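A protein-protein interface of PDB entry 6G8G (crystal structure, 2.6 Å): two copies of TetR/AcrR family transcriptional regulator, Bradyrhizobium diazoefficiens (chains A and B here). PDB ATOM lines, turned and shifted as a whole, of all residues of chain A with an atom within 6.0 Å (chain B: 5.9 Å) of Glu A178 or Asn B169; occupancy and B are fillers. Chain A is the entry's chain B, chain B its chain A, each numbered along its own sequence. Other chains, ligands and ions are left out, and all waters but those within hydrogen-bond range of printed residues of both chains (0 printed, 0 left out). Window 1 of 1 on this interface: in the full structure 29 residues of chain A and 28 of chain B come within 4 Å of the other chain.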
ATOM      1  N   SER A 173     -28.231 -23.816  27.839  1.00  0.00           N
ATOM      2  CA  SER A 173     -27.220 -24.233  26.881  1.00  0.00           C
ATOM      3  C   SER A 173     -27.731 -24.178  25.451  1.00  0.00           C
ATOM      4  O   SER A 173     -26.995 -23.805  24.560  1.00  0.00           O
ATOM      5  CB  SER A 173     -26.713 -25.626  27.218  1.00  0.00           C
ATOM      6  OG  SER A 173     -26.155 -25.594  28.520  1.00  0.00           O
ATOM      7  N   ARG A 176     -28.301 -20.360  24.418  1.00  0.00           N
ATOM      8  CA  ARG A 176     -27.016 -19.670  24.428  1.00  0.00           C
ATOM      9  C   ARG A 176     -26.124 -20.179  23.306  1.00  0.00           C
ATOM     10  O   ARG A 176     -25.472 -19.427  22.606  1.00  0.00           O
ATOM     11  CB  ARG A 176     -26.353 -20.007  25.747  1.00  0.00           C
ATOM     12  CG  ARG A 176     -25.023 -19.353  26.004  1.00  0.00           C
ATOM     13  CD  ARG A 176     -24.595 -19.539  27.442  1.00  0.00           C
ATOM     14  NE  ARG A 176     -24.198 -20.909  27.692  1.00  0.00           N
ATOM     15  CZ  ARG A 176     -24.734 -21.703  28.609  1.00  0.00           C
ATOM     16  NH1 ARG A 176     -25.702 -21.291  29.403  1.00  0.00           N
ATOM     17  NH2 ARG A 176     -24.285 -22.941  28.741  1.00  0.00           N
ATOM     18  N   GLY A 177     -26.143 -21.493  23.132  1.00  0.00           N
ATOM     19  CA  GLY A 177     -25.309 -22.174  22.161  1.00  0.00           C
ATOM     20  C   GLY A 177     -23.865 -21.764  22.226  1.00  0.00           C
ATOM     21  O   GLY A 177     -23.201 -21.927  23.222  1.00  0.00           O
ATOM     22  N   GLU A 178     -23.440 -21.120  21.170  1.00  0.00           N
ATOM     23  CA  GLU A 178     -22.042 -20.895  20.862  1.00  0.00           C
ATOM     24  C   GLU A 178     -21.639 -19.448  21.040  1.00  0.00           C
ATOM     25  O   GLU A 178     -20.528 -19.029  20.741  1.00  0.00           O
ATOM     26  CB  GLU A 178     -21.936 -21.229  19.408  1.00  0.00           C
ATOM     27  CG  GLU A 178     -20.858 -22.206  19.062  1.00  0.00           C
ATOM     28  CD  GLU A 178     -20.686 -22.291  17.562  1.00  0.00           C
ATOM     29  OE1 GLU A 178     -21.538 -21.709  16.789  1.00  0.00           O
ATOM     30  OE2 GLU A 178     -19.690 -22.949  17.188  1.00  0.00           O
ATOM     31  N   LEU A 179     -22.572 -18.671  21.533  1.00  0.00           N
ATOM     32  CA  LEU A 179     -22.446 -17.252  21.480  1.00  0.00           C
ATOM     33  C   LEU A 179     -21.317 -16.694  22.351  1.00  0.00           C
ATOM     34  O   LEU A 179     -20.630 -15.757  21.978  1.00  0.00           O
ATOM     35  CB  LEU A 179     -23.815 -16.672  21.743  1.00  0.00           C
ATOM     36  CG  LEU A 179     -23.926 -15.231  22.210  1.00  0.00           C
ATOM     37  CD1 LEU A 179     -25.129 -14.607  21.556  1.00  0.00           C
ATOM     38  CD2 LEU A 179     -24.077 -15.170  23.722  1.00  0.00           C
ATOM     39  N   PRO A 180     -21.070 -17.300  23.496  1.00  0.00           N
ATOM     40  CA  PRO A 180     -19.995 -16.744  24.327  1.00  0.00           C
ATOM     41  C   PRO A 180     -18.680 -16.734  23.557  1.00  0.00           C
ATOM     42  O   PRO A 180     -17.880 -15.787  23.658  1.00  0.00           O
ATOM     43  CB  PRO A 180     -19.921 -17.720  25.490  1.00  0.00           C
ATOM     44  CG  PRO A 180     -21.266 -18.361  25.551  1.00  0.00           C
ATOM     45  CD  PRO A 180     -21.884 -18.300  24.199  1.00  0.00           C
ATOM     46  N   LEU A 181     -18.444 -17.821  22.840  1.00  0.00           N
ATOM     47  CA  LEU A 181     -17.236 -17.927  22.052  1.00  0.00           C
ATOM     48  C   LEU A 181     -17.224 -16.881  20.949  1.00  0.00           C
ATOM     49  O   LEU A 181     -16.229 -16.202  20.733  1.00  0.00           O
ATOM     50  CB  LEU A 181     -17.146 -19.311  21.415  1.00  0.00           C
ATOM     51  CG  LEU A 181     -15.977 -19.498  20.456  1.00  0.00           C
ATOM     52  CD1 LEU A 181     -14.671 -19.541  21.217  1.00  0.00           C
ATOM     53  CD2 LEU A 181     -16.182 -20.756  19.652  1.00  0.00           C
ATOM     54  N   LEU A 182     -18.318 -16.801  20.213  1.00  0.00           N
ATOM     55  CA  LEU A 182     -18.399 -15.836  19.153  1.00  0.00           C
ATOM     56  C   LEU A 182     -18.106 -14.411  19.683  1.00  0.00           C
ATOM     57  O   LEU A 182     -17.450 -13.610  19.033  1.00  0.00           O
ATOM     58  CB  LEU A 182     -19.780 -15.926  18.504  1.00  0.00           C
ATOM     59  CG  LEU A 182     -19.975 -17.227  17.730  1.00  0.00           C
ATOM     60  CD1 LEU A 182     -21.393 -17.439  17.260  1.00  0.00           C
ATOM     61  CD2 LEU A 182     -19.056 -17.253  16.511  1.00  0.00           C
ATOM     62  N   ILE A 183     -18.628 -14.095  20.860  1.00  0.00           N
ATOM     63  CA  ILE A 183     -18.516 -12.751  21.405  1.00  0.00           C
ATOM     64  C   ILE A 183     -17.071 -12.447  21.722  1.00  0.00           C
ATOM     65  O   ILE A 183     -16.535 -11.418  21.342  1.00  0.00           O
ATOM     66  CB  ILE A 183     -19.374 -12.617  22.679  1.00  0.00           C
ATOM     67  CG1 ILE A 183     -20.848 -12.498  22.289  1.00  0.00           C
ATOM     68  CG2 ILE A 183     -18.960 -11.416  23.492  1.00  0.00           C
ATOM     69  CD1 ILE A 183     -21.783 -12.680  23.463  1.00  0.00           C
ATOM     70  N   TYR B 135     -12.344 -19.816  13.893  1.00  0.00           N
ATOM     71  CA  TYR B 135     -13.677 -20.356  14.106  1.00  0.00           C
ATOM     72  C   TYR B 135     -14.044 -21.434  13.082  1.00  0.00           C
ATOM     73  O   TYR B 135     -14.514 -22.499  13.467  1.00  0.00           O
ATOM     74  CB  TYR B 135     -14.735 -19.261  14.102  1.00  0.00           C
ATOM     75  CG  TYR B 135     -16.119 -19.826  14.294  1.00  0.00           C
ATOM     76  CD1 TYR B 135     -16.546 -20.272  15.536  1.00  0.00           C
ATOM     77  CD2 TYR B 135     -16.965 -19.978  13.215  1.00  0.00           C
ATOM     78  CE1 TYR B 135     -17.796 -20.827  15.699  1.00  0.00           C
ATOM     79  CE2 TYR B 135     -18.215 -20.543  13.346  1.00  0.00           C
ATOM     80  CZ  TYR B 135     -18.631 -20.965  14.588  1.00  0.00           C
ATOM     81  OH  TYR B 135     -19.890 -21.530  14.653  1.00  0.00           O
ATOM     82  N   PRO B 139     -13.931 -25.024  15.793  1.00  0.00           N
ATOM     83  CA  PRO B 139     -15.292 -25.206  16.238  1.00  0.00           C
ATOM     84  C   PRO B 139     -16.274 -25.543  15.124  1.00  0.00           C
ATOM     85  O   PRO B 139     -17.037 -26.503  15.246  1.00  0.00           O
ATOM     86  CB  PRO B 139     -15.628 -23.845  16.829  1.00  0.00           C
ATOM     87  CG  PRO B 139     -14.350 -23.339  17.342  1.00  0.00           C
ATOM     88  CD  PRO B 139     -13.295 -23.842  16.402  1.00  0.00           C
ATOM     89  N   GLU B 140     -16.294 -24.756  14.051  1.00  0.00           N
ATOM     90  CA  GLU B 140     -17.270 -25.031  13.003  1.00  0.00           C
ATOM     91  C   GLU B 140     -16.936 -26.339  12.322  1.00  0.00           C
ATOM     92  O   GLU B 140     -17.813 -27.049  11.873  1.00  0.00           O
ATOM     93  CB  GLU B 140     -17.375 -23.895  11.994  1.00  0.00           C
ATOM     94  CG  GLU B 140     -18.653 -23.988  11.189  1.00  0.00           C
ATOM     95  CD  GLU B 140     -18.937 -22.776  10.326  1.00  0.00           C
ATOM     96  OE1 GLU B 140     -19.840 -21.958  10.694  1.00  0.00           O
ATOM     97  OE2 GLU B 140     -18.279 -22.662   9.272  1.00  0.00           O
ATOM     98  N   ILE B 143     -18.471 -29.089  14.240  1.00  0.00           N
ATOM     99  CA  ILE B 143     -19.888 -29.186  13.928  1.00  0.00           C
ATOM    100  C   ILE B 143     -20.132 -29.933  12.601  1.00  0.00           C
ATOM    101  O   ILE B 143     -20.966 -30.823  12.547  1.00  0.00           O
ATOM    102  CB  ILE B 143     -20.517 -27.789  13.865  1.00  0.00           C
ATOM    103  CG1 ILE B 143     -20.594 -27.172  15.258  1.00  0.00           C
ATOM    104  CG2 ILE B 143     -21.909 -27.830  13.245  1.00  0.00           C
ATOM    105  CD1 ILE B 143     -20.972 -25.693  15.249  1.00  0.00           C
ATOM    106  N   LEU B 146     -19.678 -33.757  12.760  1.00  0.00           N
ATOM    107  CA  LEU B 146     -20.744 -34.423  13.467  1.00  0.00           C
ATOM    108  C   LEU B 146     -21.967 -34.404  12.595  1.00  0.00           C
ATOM    109  O   LEU B 146     -22.713 -35.361  12.543  1.00  0.00           O
ATOM    110  CB  LEU B 146     -21.005 -33.731  14.792  1.00  0.00           C
ATOM    111  CG  LEU B 146     -22.125 -34.360  15.604  1.00  0.00           C
ATOM    112  CD1 LEU B 146     -21.873 -35.824  15.840  1.00  0.00           C
ATOM    113  CD2 LEU B 146     -22.277 -33.639  16.928  1.00  0.00           C
ATOM    114  N   PRO B 164     -28.971 -30.798   9.786  1.00  0.00           N
ATOM    115  CA  PRO B 164     -27.916 -31.528  10.474  1.00  0.00           C
ATOM    116  C   PRO B 164     -26.902 -30.658  11.220  1.00  0.00           C
ATOM    117  O   PRO B 164     -26.431 -31.049  12.285  1.00  0.00           O
ATOM    118  CB  PRO B 164     -27.233 -32.297   9.346  1.00  0.00           C
ATOM    119  CG  PRO B 164     -27.608 -31.577   8.100  1.00  0.00           C
ATOM    120  CD  PRO B 164     -28.994 -31.104   8.356  1.00  0.00           C
ATOM    121  N   MET B 165     -26.613 -29.472  10.713  1.00  0.00           N
ATOM    122  CA  MET B 165     -25.713 -28.566  11.434  1.00  0.00           C
ATOM    123  C   MET B 165     -26.374 -28.030  12.684  1.00  0.00           C
ATOM    124  O   MET B 165     -25.766 -27.985  13.740  1.00  0.00           O
ATOM    125  CB  MET B 165     -25.260 -27.464  10.498  1.00  0.00           C
ATOM    126  CG  MET B 165     -24.246 -28.105   9.566  1.00  0.00           C
ATOM    127  SD  MET B 165     -23.149 -26.735   8.671  1.00  0.00           S
ATOM    128  CE  MET B 165     -22.250 -25.856  10.173  1.00  0.00           C
ATOM    129  N   GLU B 166     -27.627 -27.625  12.564  1.00  0.00           N
ATOM    130  CA  GLU B 166     -28.370 -27.191  13.696  1.00  0.00           C
ATOM    131  C   GLU B 166     -28.336 -28.294  14.735  1.00  0.00           C
ATOM    132  O   GLU B 166     -28.085 -28.039  15.897  1.00  0.00           O
ATOM    133  CB  GLU B 166     -29.801 -26.830  13.266  1.00  0.00           C
ATOM    134  CG  GLU B 166     -30.717 -26.305  14.377  1.00  0.00           C
ATOM    135  CD  GLU B 166     -32.025 -25.704  13.872  1.00  0.00           C
ATOM    136  OE1 GLU B 166     -32.862 -26.447  13.280  1.00  0.00           O
ATOM    137  OE2 GLU B 166     -32.188 -24.470  14.063  1.00  0.00           O
ATOM    138  N   ALA B 167     -28.581 -29.527  14.318  1.00  0.00           N
ATOM    139  CA  ALA B 167     -28.662 -30.631  15.283  1.00  0.00           C
ATOM    140  C   ALA B 167     -27.318 -30.923  15.889  1.00  0.00           C
ATOM    141  O   ALA B 167     -27.213 -31.215  17.064  1.00  0.00           O
ATOM    142  CB  ALA B 167     -29.210 -31.874  14.637  1.00  0.00           C
ATOM    143  N   ALA B 168     -26.280 -30.841  15.087  1.00  0.00           N
ATOM    144  CA  ALA B 168     -24.944 -31.070  15.600  1.00  0.00           C
ATOM    145  C   ALA B 168     -24.641 -30.030  16.656  1.00  0.00           C
ATOM    146  O   ALA B 168     -24.130 -30.334  17.728  1.00  0.00           O
ATOM    147  CB  ALA B 168     -23.928 -31.001  14.473  1.00  0.00           C
ATOM    148  N   ASN B 169     -24.945 -28.787  16.346  1.00  0.00           N
ATOM    149  CA  ASN B 169     -24.642 -27.707  17.269  1.00  0.00           C
ATOM    150  C   ASN B 169     -25.425 -27.858  18.572  1.00  0.00           C
ATOM    151  O   ASN B 169     -24.949 -27.534  19.656  1.00  0.00           O
ATOM    152  CB  ASN B 169     -24.938 -26.392  16.580  1.00  0.00           C
ATOM    153  CG  ASN B 169     -24.606 -25.200  17.412  1.00  0.00           C
ATOM    154  OD1 ASN B 169     -25.467 -24.401  17.598  1.00  0.00           O
ATOM    155  ND2 ASN B 169     -23.359 -25.043  17.862  1.00  0.00           N
ATOM    156  N   GLN B 170     -26.617 -28.407  18.475  1.00  0.00           N
ATOM    157  CA  GLN B 170     -27.427 -28.593  19.647  1.00  0.00           C
ATOM    158  C   GLN B 170     -26.866 -29.682  20.508  1.00  0.00           C
ATOM    159  O   GLN B 170     -26.767 -29.533  21.721  1.00  0.00           O
ATOM    160  CB  GLN B 170     -28.849 -28.896  19.238  1.00  0.00           C
ATOM    161  CG  GLN B 170     -29.522 -27.646  18.710  1.00  0.00           C
ATOM    162  CD  GLN B 170     -30.785 -27.931  17.923  1.00  0.00           C
ATOM    163  OE1 GLN B 170     -30.952 -28.999  17.329  1.00  0.00           O
ATOM    164  NE2 GLN B 170     -31.692 -26.963  17.917  1.00  0.00           N
ATOM    165  N   PHE B 171     -26.435 -30.752  19.879  1.00  0.00           N
ATOM    166  CA  PHE B 171     -25.790 -31.842  20.619  1.00  0.00           C
ATOM    167  C   PHE B 171     -24.578 -31.353  21.394  1.00  0.00           C
ATOM    168  O   PHE B 171     -24.413 -31.652  22.561  1.00  0.00           O
ATOM    169  CB  PHE B 171     -25.372 -32.966  19.673  1.00  0.00           C
ATOM    170  CG  PHE B 171     -24.652 -34.069  20.349  1.00  0.00           C
ATOM    171  CD1 PHE B 171     -25.353 -35.048  21.018  1.00  0.00           C
ATOM    172  CD2 PHE B 171     -23.288 -34.146  20.309  1.00  0.00           C
ATOM    173  CE1 PHE B 171     -24.692 -36.081  21.642  1.00  0.00           C
ATOM    174  CE2 PHE B 171     -22.615 -35.190  20.926  1.00  0.00           C
ATOM    175  CZ  PHE B 171     -23.314 -36.153  21.594  1.00  0.00           C
ATOM    176  N   LEU B 172     -23.750 -30.567  20.732  1.00  0.00           N
ATOM    177  CA  LEU B 172     -22.538 -30.080  21.336  1.00  0.00           C
ATOM    178  C   LEU B 172     -22.819 -29.042  22.412  1.00  0.00           C
ATOM    179  O   LEU B 172     -22.237 -29.103  23.490  1.00  0.00           O
ATOM    180  CB  LEU B 172     -21.605 -29.534  20.273  1.00  0.00           C
ATOM    181  CG  LEU B 172     -21.133 -30.576  19.243  1.00  0.00           C
ATOM    182  CD1 LEU B 172     -20.534 -29.910  18.017  1.00  0.00           C
ATOM    183  CD2 LEU B 172     -20.117 -31.521  19.862  1.00  0.00           C
ATOM    184  N   SER B 173     -23.751 -28.138  22.179  1.00  0.00           N
ATOM    185  CA  SER B 173     -24.168 -27.238  23.256  1.00  0.00           C
ATOM    186  C   SER B 173     -24.680 -27.996  24.489  1.00  0.00           C
ATOM    187  O   SER B 173     -24.365 -27.614  25.590  1.00  0.00           O
ATOM    188  CB  SER B 173     -25.230 -26.289  22.775  1.00  0.00           C
ATOM    189  OG  SER B 173     -24.705 -25.566  21.680  1.00  0.00           O
ATOM    190  N   LEU B 174     -25.413 -29.086  24.301  1.00  0.00           N
ATOM    191  CA  LEU B 174     -25.907 -29.832  25.439  1.00  0.00           C
ATOM    192  C   LEU B 174     -24.798 -30.472  26.250  1.00  0.00           C
ATOM    193  O   LEU B 174     -24.775 -30.385  27.459  1.00  0.00           O
ATOM    194  CB  LEU B 174     -26.860 -30.915  25.003  1.00  0.00           C
ATOM    195  CG  LEU B 174     -28.167 -30.326  24.514  1.00  0.00           C
ATOM    196  CD1 LEU B 174     -28.961 -31.366  23.760  1.00  0.00           C
ATOM    197  CD2 LEU B 174     -28.970 -29.783  25.693  1.00  0.00           C
ATOM    198  N   ARG B 176     -21.555 -29.895  26.152  1.00  0.00           N
ATOM    199  CA  ARG B 176     -20.592 -28.905  26.619  1.00  0.00           C
ATOM    200  C   ARG B 176     -21.177 -28.176  27.804  1.00  0.00           C
ATOM    201  O   ARG B 176     -20.509 -27.911  28.767  1.00  0.00           O
ATOM    202  CB  ARG B 176     -20.358 -27.925  25.458  1.00  0.00           C
ATOM    203  CG  ARG B 176     -19.360 -26.840  25.691  1.00  0.00           C
ATOM    204  CD  ARG B 176     -19.068 -26.132  24.394  1.00  0.00           C
ATOM    205  NE  ARG B 176     -20.177 -25.298  23.973  1.00  0.00           N
ATOM    206  CZ  ARG B 176     -20.795 -25.371  22.803  1.00  0.00           C
ATOM    207  NH1 ARG B 176     -20.440 -26.258  21.899  1.00  0.00           N
ATOM    208  NH2 ARG B 176     -21.776 -24.541  22.531  1.00  0.00           N
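The guanidinium group (NH2) of Arg B176 lies within hydrogen-bond range of the backbone carbonyl oxygen (O) of Gly A177, 3.1 Å away.
The side-chain hydroxyl of Tyr B135 lies within hydrogen-bond range of the side-chain carboxylate of Glu A178, at 2.7 Å.
The side-chain hydroxyl (OG) of Ser A173 is in hydrogen-bond range of the guanidinium group (NH2) of Arg A176.
The side-chain hydroxyl of Ser B173 lies within hydrogen-bond range of the backbone carbonyl oxygen of Asn B169 (2.8 Å).
The side-chain hydroxyl (OG) of Ser B173 lies within hydrogen-bond range of the guanidinium group (NH2) of Arg B176 (3.2 Å).
N of Glu B140 lies within hydrogen-bond range of O of Tyr B135 (2.9 Å).
Among the printed residues, pairs that only touch across the chains: Gly A177 with Ser B173 (3.5 Å), Ser A173 with Ser B173 (3.5 Å), Glu A178 with Ile B143 (3.6 Å), Glu A178 with Asn B169 (3.8 Å), Leu A182 with Tyr B135 (3.9 Å) and Leu A181 with Pro B139 (3.9 Å).
Of the printed residues of chain B, Gly A177 touches Ser B173 (3.5 Å) and Arg B176 (3.1 Å).
Of the printed residues of chain B, Glu A178 touches Tyr B135, Ile B143 and Asn B169.
Of the printed residues of chain B, Leu A181 touches Pro B139.
Of the printed residues of chain A, Tyr B135 touches Glu A178 (2.7 Å) and Leu A182 (3.9 Å).
Of the printed residues of chain A, Pro B139 touches Leu A181.
Glu B140 touches none of the printed residues of chain A.
Pro B164 touches none of the printed residues of chain A.
Asn B169 touches just one residue of chain A: Glu A178.
Of the printed residues of chain A, Arg B176 touches Gly A177 (3.1 Å).
Hydrophobic or aromatic side chains of chain A within 4 Å of the printed part of chain B: Leu A181 and Leu A182.
Of the 17 printed residues of chain B, 6 touch a printed residue of chain A.
Along chain B the printed residues that touch a printed residue of chain A span positions 135 to 176.
Among the printed residues, 8 pairs touch across the chains.
Ser A173 touches its own counterpart, Ser B173.
Positions printed for both chains: 173 and 176.
Of the 8 pairs that touch across the chains among the printed residues, 1 has its exchanged pair printed and touching as well.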
